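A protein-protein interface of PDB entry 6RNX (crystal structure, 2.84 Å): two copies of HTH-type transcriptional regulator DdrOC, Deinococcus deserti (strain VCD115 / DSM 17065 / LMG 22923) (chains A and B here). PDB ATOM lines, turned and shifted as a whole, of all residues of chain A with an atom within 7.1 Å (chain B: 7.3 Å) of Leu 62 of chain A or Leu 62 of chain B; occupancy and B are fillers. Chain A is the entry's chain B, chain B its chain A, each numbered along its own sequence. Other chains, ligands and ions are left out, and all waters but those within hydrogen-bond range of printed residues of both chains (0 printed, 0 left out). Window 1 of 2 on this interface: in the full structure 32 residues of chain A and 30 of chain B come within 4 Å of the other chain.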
ATOM      1  N   LEU A   3      25.409  21.894  14.150  1.00  0.00           N
ATOM      2  CA  LEU A   3      24.468  20.799  14.081  1.00  0.00           C
ATOM      3  C   LEU A   3      23.136  21.207  13.450  1.00  0.00           C
ATOM      4  O   LEU A   3      22.485  20.388  12.798  1.00  0.00           O
ATOM      5  CB  LEU A   3      24.298  20.246  15.484  1.00  0.00           C
ATOM      6  CG  LEU A   3      23.245  19.204  15.789  1.00  0.00           C
ATOM      7  CD1 LEU A   3      23.416  18.024  14.883  1.00  0.00           C
ATOM      8  CD2 LEU A   3      23.428  18.786  17.234  1.00  0.00           C
ATOM      9  N   ARG A   6      23.790  21.131   9.702  1.00  0.00           N
ATOM     10  CA  ARG A   6      23.943  19.762   9.207  1.00  0.00           C
ATOM     11  C   ARG A   6      22.599  19.098   9.036  1.00  0.00           C
ATOM     12  O   ARG A   6      22.349  18.450   8.011  1.00  0.00           O
ATOM     13  CB  ARG A   6      24.812  18.926  10.146  1.00  0.00           C
ATOM     14  CG  ARG A   6      25.094  17.509   9.628  1.00  0.00           C
ATOM     15  CD  ARG A   6      26.481  17.371   8.982  1.00  0.00           C
ATOM     16  NE  ARG A   6      26.801  15.993   8.606  1.00  0.00           N
ATOM     17  CZ  ARG A   6      26.606  15.469   7.395  1.00  0.00           C
ATOM     18  NH1 ARG A   6      26.095  16.204   6.410  1.00  0.00           N
ATOM     19  NH2 ARG A   6      26.922  14.201   7.167  1.00  0.00           N
ATOM     20  N   LEU A   7      21.723  19.256  10.039  1.00  0.00           N
ATOM     21  CA  LEU A   7      20.384  18.693   9.971  1.00  0.00           C
ATOM     22  C   LEU A   7      19.588  19.316   8.843  1.00  0.00           C
ATOM     23  O   LEU A   7      18.763  18.635   8.225  1.00  0.00           O
ATOM     24  CB  LEU A   7      19.672  18.868  11.311  1.00  0.00           C
ATOM     25  CG  LEU A   7      20.334  18.145  12.496  1.00  0.00           C
ATOM     26  CD1 LEU A   7      19.963  18.791  13.815  1.00  0.00           C
ATOM     27  CD2 LEU A   7      19.999  16.661  12.543  1.00  0.00           C
ATOM     28  N   LEU A  10      21.230  17.687   5.410  1.00  0.00           N
ATOM     29  CA  LEU A  10      20.783  16.343   5.068  1.00  0.00           C
ATOM     30  C   LEU A  10      19.425  16.374   4.385  1.00  0.00           C
ATOM     31  O   LEU A  10      19.260  15.826   3.292  1.00  0.00           O
ATOM     32  CB  LEU A  10      20.758  15.476   6.325  1.00  0.00           C
ATOM     33  CG  LEU A  10      22.177  15.396   6.889  1.00  0.00           C
ATOM     34  CD1 LEU A  10      22.198  14.738   8.248  1.00  0.00           C
ATOM     35  CD2 LEU A  10      23.081  14.672   5.923  1.00  0.00           C
ATOM     36  N   LEU A  44      19.649  12.974  22.583  1.00  0.00           N
ATOM     37  CA  LEU A  44      20.280  11.884  21.842  1.00  0.00           C
ATOM     38  C   LEU A  44      19.241  10.897  21.338  1.00  0.00           C
ATOM     39  O   LEU A  44      19.447  10.247  20.304  1.00  0.00           O
ATOM     40  CB  LEU A  44      21.314  11.173  22.705  1.00  0.00           C
ATOM     41  CG  LEU A  44      22.416  12.070  23.259  1.00  0.00           C
ATOM     42  CD1 LEU A  44      23.222  11.354  24.358  1.00  0.00           C
ATOM     43  CD2 LEU A  44      23.311  12.518  22.136  1.00  0.00           C
ATOM     44  N   LEU A  47      18.281  12.748  18.076  1.00  0.00           N
ATOM     45  CA  LEU A  47      19.328  12.618  17.075  1.00  0.00           C
ATOM     46  C   LEU A  47      19.258  11.274  16.362  1.00  0.00           C
ATOM     47  O   LEU A  47      19.213  11.226  15.130  1.00  0.00           O
ATOM     48  CB  LEU A  47      20.687  12.803  17.729  1.00  0.00           C
ATOM     49  CG  LEU A  47      21.358  14.150  17.498  1.00  0.00           C
ATOM     50  CD1 LEU A  47      22.823  14.040  17.872  1.00  0.00           C
ATOM     51  CD2 LEU A  47      21.176  14.610  16.061  1.00  0.00           C
ATOM     52  N   ILE A  56      21.806   7.107   7.586  1.00  0.00           N
ATOM     53  CA  ILE A  56      23.151   7.124   8.150  1.00  0.00           C
ATOM     54  C   ILE A  56      23.066   6.853   9.649  1.00  0.00           C
ATOM     55  O   ILE A  56      21.970   6.764  10.213  1.00  0.00           O
ATOM     56  CB  ILE A  56      23.848   8.466   7.867  1.00  0.00           C
ATOM     57  CG1 ILE A  56      23.195   9.567   8.703  1.00  0.00           C
ATOM     58  CG2 ILE A  56      23.846   8.765   6.344  1.00  0.00           C
ATOM     59  CD1 ILE A  56      23.740  10.911   8.451  1.00  0.00           C
ATOM     60  N   THR A  57      24.216   6.714  10.301  1.00  0.00           N
ATOM     61  CA  THR A  57      24.282   6.485  11.732  1.00  0.00           C
ATOM     62  C   THR A  57      24.451   7.820  12.452  1.00  0.00           C
ATOM     63  O   THR A  57      24.549   8.871  11.821  1.00  0.00           O
ATOM     64  CB  THR A  57      25.415   5.518  12.052  1.00  0.00           C
ATOM     65  OG1 THR A  57      25.252   5.030  13.388  1.00  0.00           O
ATOM     66  CG2 THR A  57      26.746   6.216  11.926  1.00  0.00           C
ATOM     67  N   VAL A  58      24.475   7.792  13.790  1.00  0.00           N
ATOM     68  CA  VAL A  58      24.634   9.053  14.519  1.00  0.00           C
ATOM     69  C   VAL A  58      26.079   9.523  14.474  1.00  0.00           C
ATOM     70  O   VAL A  58      26.343  10.722  14.359  1.00  0.00           O
ATOM     71  CB  VAL A  58      24.117   8.940  15.963  1.00  0.00           C
ATOM     72  CG1 VAL A  58      24.626  10.099  16.770  1.00  0.00           C
ATOM     73  CG2 VAL A  58      22.600   8.991  15.990  1.00  0.00           C
ATOM     74  N   HIS A  59      27.034   8.589  14.560  1.00  0.00           N
ATOM     75  CA  HIS A  59      28.439   8.905  14.320  1.00  0.00           C
ATOM     76  C   HIS A  59      28.594   9.681  13.018  1.00  0.00           C
ATOM     77  O   HIS A  59      29.066  10.823  13.008  1.00  0.00           O
ATOM     78  CB  HIS A  59      29.264   7.607  14.296  1.00  0.00           C
ATOM     79  CG  HIS A  59      30.722   7.807  13.998  1.00  0.00           C
ATOM     80  ND1 HIS A  59      31.414   7.011  13.111  1.00  0.00           N
ATOM     81  CD2 HIS A  59      31.621   8.702  14.473  1.00  0.00           C
ATOM     82  CE1 HIS A  59      32.672   7.407  13.046  1.00  0.00           C
ATOM     83  NE2 HIS A  59      32.825   8.432  13.864  1.00  0.00           N
ATOM     84  N   ASP A  60      28.150   9.084  11.910  1.00  0.00           N
ATOM     85  CA  ASP A  60      28.306   9.702  10.595  1.00  0.00           C
ATOM     86  C   ASP A  60      27.599  11.055  10.512  1.00  0.00           C
ATOM     87  O   ASP A  60      28.099  11.992   9.876  1.00  0.00           O
ATOM     88  CB  ASP A  60      27.765   8.756   9.520  1.00  0.00           C
ATOM     89  CG  ASP A  60      28.671   7.559   9.274  1.00  0.00           C
ATOM     90  OD1 ASP A  60      29.274   7.034  10.242  1.00  0.00           O
ATOM     91  OD2 ASP A  60      28.766   7.142   8.097  1.00  0.00           O
ATOM     92  N   LEU A  61      26.424  11.174  11.129  1.00  0.00           N
ATOM     93  CA  LEU A  61      25.681  12.429  11.065  1.00  0.00           C
ATOM     94  C   LEU A  61      26.507  13.583  11.610  1.00  0.00           C
ATOM     95  O   LEU A  61      26.512  14.679  11.041  1.00  0.00           O
ATOM     96  CB  LEU A  61      24.364  12.285  11.822  1.00  0.00           C
ATOM     97  CG  LEU A  61      23.299  13.378  11.792  1.00  0.00           C
ATOM     98  CD1 LEU A  61      21.947  12.747  11.982  1.00  0.00           C
ATOM     99  CD2 LEU A  61      23.521  14.436  12.875  1.00  0.00           C
ATOM    100  N   LEU A  62      27.222  13.352  12.696  1.00  0.00           N
ATOM    101  CA  LEU A  62      28.069  14.370  13.287  1.00  0.00           C
ATOM    102  C   LEU A  62      29.438  14.473  12.618  1.00  0.00           C
ATOM    103  O   LEU A  62      30.320  15.174  13.143  1.00  0.00           O
ATOM    104  CB  LEU A  62      28.213  14.106  14.782  1.00  0.00           C
ATOM    105  CG  LEU A  62      26.827  13.926  15.356  1.00  0.00           C
ATOM    106  CD1 LEU A  62      26.916  13.480  16.780  1.00  0.00           C
ATOM    107  CD2 LEU A  62      26.116  15.234  15.250  1.00  0.00           C
ATOM    108  N   GLU A  63      29.626  13.801  11.484  1.00  0.00           N
ATOM    109  CA  GLU A  63      30.839  13.938  10.680  1.00  0.00           C
ATOM    110  C   GLU A  63      30.738  15.275   9.957  1.00  0.00           C
ATOM    111  O   GLU A  63      29.970  15.439   9.007  1.00  0.00           O
ATOM    112  CB  GLU A  63      30.987  12.752   9.732  1.00  0.00           C
ATOM    113  CG  GLU A  63      31.731  12.979   8.425  1.00  0.00           C
ATOM    114  CD  GLU A  63      31.621  11.774   7.488  1.00  0.00           C
ATOM    115  OE1 GLU A  63      32.451  10.838   7.600  1.00  0.00           O
ATOM    116  OE2 GLU A  63      30.687  11.758   6.651  1.00  0.00           O
ATOM    117  N   GLY A  64      31.479  16.257  10.450  1.00  0.00           N
ATOM    118  CA  GLY A  64      31.358  17.602   9.938  1.00  0.00           C
ATOM    119  C   GLY A  64      31.054  18.622  11.015  1.00  0.00           C
ATOM    120  O   GLY A  64      31.709  19.663  11.100  1.00  0.00           O
ATOM    121  N   VAL A  65      30.054  18.344  11.849  1.00  0.00           N
ATOM    122  CA  VAL A  65      29.614  19.353  12.806  1.00  0.00           C
ATOM    123  C   VAL A  65      30.688  19.555  13.863  1.00  0.00           C
ATOM    124  O   VAL A  65      31.579  18.732  14.040  1.00  0.00           O
ATOM    125  CB  VAL A  65      28.270  18.953  13.437  1.00  0.00           C
ATOM    126  CG1 VAL A  65      27.342  18.444  12.365  1.00  0.00           C
ATOM    127  CG2 VAL A  65      28.462  17.892  14.503  1.00  0.00           C
ATOM    128  N   GLU A  66      30.616  20.685  14.556  1.00  0.00           N
ATOM    129  CA  GLU A  66      31.480  20.887  15.706  1.00  0.00           C
ATOM    130  C   GLU A  66      30.799  21.793  16.721  1.00  0.00           C
ATOM    131  O   GLU A  66      29.805  22.459  16.425  1.00  0.00           O
ATOM    132  CB  GLU A  66      32.842  21.443  15.301  1.00  0.00           C
ATOM    133  CG  GLU A  66      33.969  20.763  16.066  1.00  0.00           C
ATOM    134  CD  GLU A  66      35.279  20.788  15.321  1.00  0.00           C
ATOM    135  OE1 GLU A  66      35.255  20.931  14.079  1.00  0.00           O
ATOM    136  OE2 GLU A  66      36.334  20.682  15.983  1.00  0.00           O
ATOM    137  N   PHE A  67      31.357  21.794  17.934  1.00  0.00           N
ATOM    138  CA  PHE A  67      30.759  22.404  19.116  1.00  0.00           C
ATOM    139  C   PHE A  67      31.789  23.262  19.839  1.00  0.00           C
ATOM    140  O   PHE A  67      33.004  23.089  19.668  1.00  0.00           O
ATOM    141  CB  PHE A  67      30.228  21.347  20.099  1.00  0.00           C
ATOM    142  CG  PHE A  67      29.361  20.278  19.471  1.00  0.00           C
ATOM    143  CD1 PHE A  67      29.928  19.173  18.843  1.00  0.00           C
ATOM    144  CD2 PHE A  67      27.968  20.359  19.554  1.00  0.00           C
ATOM    145  CE1 PHE A  67      29.121  18.191  18.278  1.00  0.00           C
ATOM    146  CE2 PHE A  67      27.147  19.373  18.992  1.00  0.00           C
ATOM    147  CZ  PHE A  67      27.720  18.296  18.352  1.00  0.00           C
ATOM    148  N   LEU B   3      26.451   3.986  25.024  1.00  0.00           N
ATOM    149  CA  LEU B   3      27.242   5.191  25.241  1.00  0.00           C
ATOM    150  C   LEU B   3      27.889   5.202  26.620  1.00  0.00           C
ATOM    151  O   LEU B   3      28.997   5.726  26.766  1.00  0.00           O
ATOM    152  CB  LEU B   3      26.381   6.438  25.028  1.00  0.00           C
ATOM    153  CG  LEU B   3      26.978   7.802  25.377  1.00  0.00           C
ATOM    154  CD1 LEU B   3      28.286   8.106  24.647  1.00  0.00           C
ATOM    155  CD2 LEU B   3      25.935   8.839  25.046  1.00  0.00           C
ATOM    156  N   ARG B   6      31.146   3.385  26.574  1.00  0.00           N
ATOM    157  CA  ARG B   6      32.167   4.141  25.864  1.00  0.00           C
ATOM    158  C   ARG B   6      32.762   5.225  26.748  1.00  0.00           C
ATOM    159  O   ARG B   6      33.978   5.451  26.742  1.00  0.00           O
ATOM    160  CB  ARG B   6      31.534   4.758  24.620  1.00  0.00           C
ATOM    161  CG  ARG B   6      32.389   5.744  23.894  1.00  0.00           C
ATOM    162  CD  ARG B   6      33.493   5.037  23.159  1.00  0.00           C
ATOM    163  NE  ARG B   6      34.176   5.959  22.267  1.00  0.00           N
ATOM    164  CZ  ARG B   6      35.421   5.805  21.848  1.00  0.00           C
ATOM    165  NH1 ARG B   6      36.139   4.750  22.229  1.00  0.00           N
ATOM    166  NH2 ARG B   6      35.931   6.712  21.041  1.00  0.00           N
ATOM    167  N   LEU B   7      31.910   5.911  27.509  1.00  0.00           N
ATOM    168  CA  LEU B   7      32.362   6.990  28.374  1.00  0.00           C
ATOM    169  C   LEU B   7      33.215   6.478  29.510  1.00  0.00           C
ATOM    170  O   LEU B   7      34.047   7.223  30.032  1.00  0.00           O
ATOM    171  CB  LEU B   7      31.165   7.744  28.947  1.00  0.00           C
ATOM    172  CG  LEU B   7      30.215   8.397  27.944  1.00  0.00           C
ATOM    173  CD1 LEU B   7      28.904   8.774  28.612  1.00  0.00           C
ATOM    174  CD2 LEU B   7      30.883   9.597  27.297  1.00  0.00           C
ATOM    175  N   LEU B  10      36.717   5.418  27.828  1.00  0.00           N
ATOM    176  CA  LEU B  10      37.601   6.531  27.501  1.00  0.00           C
ATOM    177  C   LEU B  10      38.403   6.973  28.717  1.00  0.00           C
ATOM    178  O   LEU B  10      39.599   7.272  28.604  1.00  0.00           O
ATOM    179  CB  LEU B  10      36.787   7.690  26.927  1.00  0.00           C
ATOM    180  CG  LEU B  10      36.244   7.502  25.508  1.00  0.00           C
ATOM    181  CD1 LEU B  10      35.175   8.538  25.152  1.00  0.00           C
ATOM    182  CD2 LEU B  10      37.384   7.588  24.525  1.00  0.00           C
ATOM    183  N   LEU B  44      23.747  17.012  24.931  1.00  0.00           N
ATOM    184  CA  LEU B  44      24.869  17.267  24.038  1.00  0.00           C
ATOM    185  C   LEU B  44      25.887  18.172  24.711  1.00  0.00           C
ATOM    186  O   LEU B  44      27.101  17.985  24.556  1.00  0.00           O
ATOM    187  CB  LEU B  44      24.386  17.894  22.735  1.00  0.00           C
ATOM    188  CG  LEU B  44      23.650  17.004  21.747  1.00  0.00           C
ATOM    189  CD1 LEU B  44      22.908  17.838  20.686  1.00  0.00           C
ATOM    190  CD2 LEU B  44      24.657  16.077  21.115  1.00  0.00           C
ATOM    191  N   LEU B  47      28.087  16.357  26.762  1.00  0.00           N
ATOM    192  CA  LEU B  47      29.010  15.562  25.951  1.00  0.00           C
ATOM    193  C   LEU B  47      30.183  16.401  25.444  1.00  0.00           C
ATOM    194  O   LEU B  47      31.315  15.909  25.386  1.00  0.00           O
ATOM    195  CB  LEU B  47      28.273  14.901  24.783  1.00  0.00           C
ATOM    196  CG  LEU B  47      27.759  13.453  24.913  1.00  0.00           C
ATOM    197  CD1 LEU B  47      27.329  12.895  23.566  1.00  0.00           C
ATOM    198  CD2 LEU B  47      28.774  12.519  25.549  1.00  0.00           C
ATOM    199  N   ILE B  56      39.224  14.786  22.705  1.00  0.00           N
ATOM    200  CA  ILE B  56      38.573  14.091  21.609  1.00  0.00           C
ATOM    201  C   ILE B  56      37.431  14.975  21.110  1.00  0.00           C
ATOM    202  O   ILE B  56      36.869  15.772  21.870  1.00  0.00           O
ATOM    203  CB  ILE B  56      38.057  12.714  22.099  1.00  0.00           C
ATOM    204  CG1 ILE B  56      39.165  11.858  22.740  1.00  0.00           C
ATOM    205  CG2 ILE B  56      37.445  11.946  20.992  1.00  0.00           C
ATOM    206  CD1 ILE B  56      40.507  11.816  22.001  1.00  0.00           C
ATOM    207  N   THR B  57      37.098  14.859  19.825  1.00  0.00           N
ATOM    208  CA  THR B  57      35.908  15.553  19.353  1.00  0.00           C
ATOM    209  C   THR B  57      34.680  14.764  19.771  1.00  0.00           C
ATOM    210  O   THR B  57      34.773  13.610  20.186  1.00  0.00           O
ATOM    211  CB  THR B  57      35.928  15.758  17.825  1.00  0.00           C
ATOM    212  OG1 THR B  57      35.362  14.626  17.140  1.00  0.00           O
ATOM    213  CG2 THR B  57      37.349  15.981  17.339  1.00  0.00           C
ATOM    214  N   VAL B  58      33.515  15.407  19.670  1.00  0.00           N
ATOM    215  CA  VAL B  58      32.262  14.720  19.978  1.00  0.00           C
ATOM    216  C   VAL B  58      31.934  13.697  18.893  1.00  0.00           C
ATOM    217  O   VAL B  58      31.315  12.662  19.168  1.00  0.00           O
ATOM    218  CB  VAL B  58      31.128  15.745  20.157  1.00  0.00           C
ATOM    219  CG1 VAL B  58      29.773  15.052  20.284  1.00  0.00           C
ATOM    220  CG2 VAL B  58      31.387  16.632  21.346  1.00  0.00           C
ATOM    221  N   HIS B  59      32.342  13.961  17.652  1.00  0.00           N
ATOM    222  CA  HIS B  59      32.232  12.949  16.609  1.00  0.00           C
ATOM    223  C   HIS B  59      33.032  11.706  16.985  1.00  0.00           C
ATOM    224  O   HIS B  59      32.542  10.578  16.846  1.00  0.00           O
ATOM    225  CB  HIS B  59      32.699  13.546  15.274  1.00  0.00           C
ATOM    226  CG  HIS B  59      32.874  12.551  14.162  1.00  0.00           C
ATOM    227  ND1 HIS B  59      34.108  12.063  13.788  1.00  0.00           N
ATOM    228  CD2 HIS B  59      31.979  11.990  13.314  1.00  0.00           C
ATOM    229  CE1 HIS B  59      33.961  11.227  12.777  1.00  0.00           C
ATOM    230  NE2 HIS B  59      32.679  11.168  12.466  1.00  0.00           N
ATOM    231  N   ASP B  60      34.246  11.898  17.514  1.00  0.00           N
ATOM    232  CA  ASP B  60      35.147  10.780  17.778  1.00  0.00           C
ATOM    233  C   ASP B  60      34.730  10.004  19.020  1.00  0.00           C
ATOM    234  O   ASP B  60      34.829   8.771  19.052  1.00  0.00           O
ATOM    235  CB  ASP B  60      36.581  11.292  17.922  1.00  0.00           C
ATOM    236  CG  ASP B  60      37.302  11.397  16.605  1.00  0.00           C
ATOM    237  OD1 ASP B  60      36.640  11.623  15.574  1.00  0.00           O
ATOM    238  OD2 ASP B  60      38.541  11.248  16.602  1.00  0.00           O
ATOM    239  N   LEU B  61      34.286  10.720  20.054  1.00  0.00           N
ATOM    240  CA  LEU B  61      33.685  10.096  21.227  1.00  0.00           C
ATOM    241  C   LEU B  61      32.597   9.107  20.837  1.00  0.00           C
ATOM    242  O   LEU B  61      32.513   8.009  21.396  1.00  0.00           O
ATOM    243  CB  LEU B  61      33.111  11.184  22.134  1.00  0.00           C
ATOM    244  CG  LEU B  61      32.783  10.864  23.589  1.00  0.00           C
ATOM    245  CD1 LEU B  61      32.935  12.097  24.453  1.00  0.00           C
ATOM    246  CD2 LEU B  61      31.375  10.330  23.688  1.00  0.00           C
ATOM    247  N   LEU B  62      31.756   9.478  19.878  1.00  0.00           N
ATOM    248  CA  LEU B  62      30.645   8.643  19.464  1.00  0.00           C
ATOM    249  C   LEU B  62      31.039   7.591  18.425  1.00  0.00           C
ATOM    250  O   LEU B  62      30.156   6.952  17.829  1.00  0.00           O
ATOM    251  CB  LEU B  62      29.512   9.525  18.940  1.00  0.00           C
ATOM    252  CG  LEU B  62      28.711  10.292  19.996  1.00  0.00           C
ATOM    253  CD1 LEU B  62      27.806  11.286  19.328  1.00  0.00           C
ATOM    254  CD2 LEU B  62      27.895   9.349  20.845  1.00  0.00           C
ATOM    255  N   GLU B  63      32.339   7.373  18.223  1.00  0.00           N
ATOM    256  CA  GLU B  63      32.780   6.399  17.235  1.00  0.00           C
ATOM    257  C   GLU B  63      32.192   5.016  17.513  1.00  0.00           C
ATOM    258  O   GLU B  63      31.441   4.473  16.694  1.00  0.00           O
ATOM    259  CB  GLU B  63      34.302   6.350  17.203  1.00  0.00           C
ATOM    260  CG  GLU B  63      34.829   5.495  16.089  1.00  0.00           C
ATOM    261  CD  GLU B  63      36.262   5.814  15.767  1.00  0.00           C
ATOM    262  OE1 GLU B  63      36.658   6.983  15.957  1.00  0.00           O
ATOM    263  OE2 GLU B  63      36.990   4.902  15.321  1.00  0.00           O
ATOM    264  N   GLY B  64      32.501   4.440  18.674  1.00  0.00           N
ATOM    265  CA  GLY B  64      32.149   3.048  18.873  1.00  0.00           C
ATOM    266  C   GLY B  64      30.713   2.729  19.253  1.00  0.00           C
ATOM    267  O   GLY B  64      30.411   1.556  19.503  1.00  0.00           O
ATOM    268  N   VAL B  65      29.812   3.708  19.287  1.00  0.00           N
ATOM    269  CA  VAL B  65      28.546   3.564  19.994  1.00  0.00           C
ATOM    270  C   VAL B  65      27.402   3.359  19.011  1.00  0.00           C
ATOM    271  O   VAL B  65      27.575   3.374  17.798  1.00  0.00           O
ATOM    272  CB  VAL B  65      28.250   4.763  20.925  1.00  0.00           C
ATOM    273  CG1 VAL B  65      29.487   5.156  21.711  1.00  0.00           C
ATOM    274  CG2 VAL B  65      27.739   5.925  20.139  1.00  0.00           C
ATOM    275  N   GLU B  66      26.217   3.155  19.574  1.00  0.00           N
ATOM    276  CA  GLU B  66      24.945   3.040  18.879  1.00  0.00           C
ATOM    277  C   GLU B  66      23.890   3.268  19.951  1.00  0.00           C
ATOM    278  O   GLU B  66      24.186   3.180  21.142  1.00  0.00           O
ATOM    279  CB  GLU B  66      24.809   1.672  18.184  1.00  0.00           C
ATOM    280  CG  GLU B  66      23.384   1.241  17.825  1.00  0.00           C
ATOM    281  CD  GLU B  66      23.064   1.389  16.351  1.00  0.00           C
ATOM    282  OE1 GLU B  66      21.984   0.923  15.942  1.00  0.00           O
ATOM    283  OE2 GLU B  66      23.885   1.966  15.606  1.00  0.00           O
ATOM    284  N   PHE B  67      22.674   3.608  19.542  1.00  0.00           N
ATOM    285  CA  PHE B  67      21.627   3.799  20.550  1.00  0.00           C
ATOM    286  C   PHE B  67      20.440   2.855  20.335  1.00  0.00           C
ATOM    287  O   PHE B  67      19.506   2.815  21.142  1.00  0.00           O
ATOM    288  CB  PHE B  67      21.131   5.251  20.570  1.00  0.00           C
ATOM    289  CG  PHE B  67      22.223   6.288  20.759  1.00  0.00           C
ATOM    290  CD1 PHE B  67      23.136   6.558  19.744  1.00  0.00           C
ATOM    291  CD2 PHE B  67      22.307   7.024  21.935  1.00  0.00           C
ATOM    292  CE1 PHE B  67      24.119   7.516  19.910  1.00  0.00           C
ATOM    293  CE2 PHE B  67      23.295   7.984  22.106  1.00  0.00           C
ATOM    294  CZ  PHE B  67      24.201   8.229  21.092  1.00  0.00           C
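NE2 of His 59 of chain B sits at hydrogen-bond distance from NE2 of His 59 of chain A (3.1 Å).
Among the printed residues, merely in contact across the chains: Glu 63 of chain A with His 59 of chain B (3.5 Å), Leu 62 of chain A with Leu 62 of chain B (3.5 Å), Leu 62 of chain A with His 59 of chain B (3.6 Å), Leu 3 of chain A with Leu 44 of chain B (3.6 Å), Phe 67 of chain A with Val 58 of chain B (3.7 Å), His 59 of chain A with Leu 62 of chain B (3.7 Å), Leu 44 of chain A with Leu 3 of chain B (3.8 Å), His 59 of chain A with Glu 63 of chain B (3.8 Å), Leu 44 of chain A with Phe 67 of chain B (3.8 Å) and Leu 44 of chain A with Leu 44 of chain B (3.9 Å).
Arg 6 of chain A touches none of the printed residues of chain B.
Of the printed residues of chain B, Leu 44 of chain A touches Leu 3, Leu 44 and Phe 67.
Of the printed residues of chain B, Phe 67 of chain A touches Val 58 (3.7 Å).
Printed residues of chain A within 4 Å of Glu 63 of chain B: His 59.
Printed residues of chain A within 4 Å of Phe 67 of chain B: Leu 44 (3.8 Å).
NE of Arg 6 of chain A is in hydrogen-bond range of O of Glu 63 of chain A (3.2 Å).
The side-chain carboxylate of Asp 60 of chain B sits at hydrogen-bond distance from a ring nitrogen (ND1) of His 59 of chain B.
The backbone NH (N) of His 59 of chain B is in hydrogen-bond range of the side-chain hydroxyl (OG1) of Thr 57 of chain B.
Leu 44 of chain A touches its own counterpart, Leu 44 of chain B.
Leu 44 of chain A touches Phe 67 of chain B, but with the chains exchanged Phe 67 of chain A does not touch Leu 44 of chain B (4.6 Å).
His 59 of chain A touches its own counterpart, His 59 of chain B.
Leu 62 of chain A touches its own counterpart, Leu 62 of chain B.
Positions printed for both chains: 3, 6, 7, 10, 44, 47, 56, 57, 58, 59, 60, 61, 62, 63, 64, 65, 66 and 67.
Of the 11 pairs that touch across the chains among the printed residues, 9 have their exchanged pair printed and touching as well.
Hydrophobic or aromatic side chains of chain B within 4 Å of the printed part of chain A: Leu 3, Leu 44, Val 58, His 59, Leu 62 and Phe 67.
Of the 18 printed residues of chain A, 6 touch a printed residue of chain B.
Hydrophobic or aromatic side chains of chain A that line the printed part of chain B: Leu 3, Leu 44, His 59, Leu 62 and Phe 67.
Along chain A the printed residues that touch a printed residue of chain B span positions 3 to 67.
Among the printed residues, no Asp or Glu carboxylate lies within 4 Å of a Lys or Arg side-chain nitrogen of the other chain.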
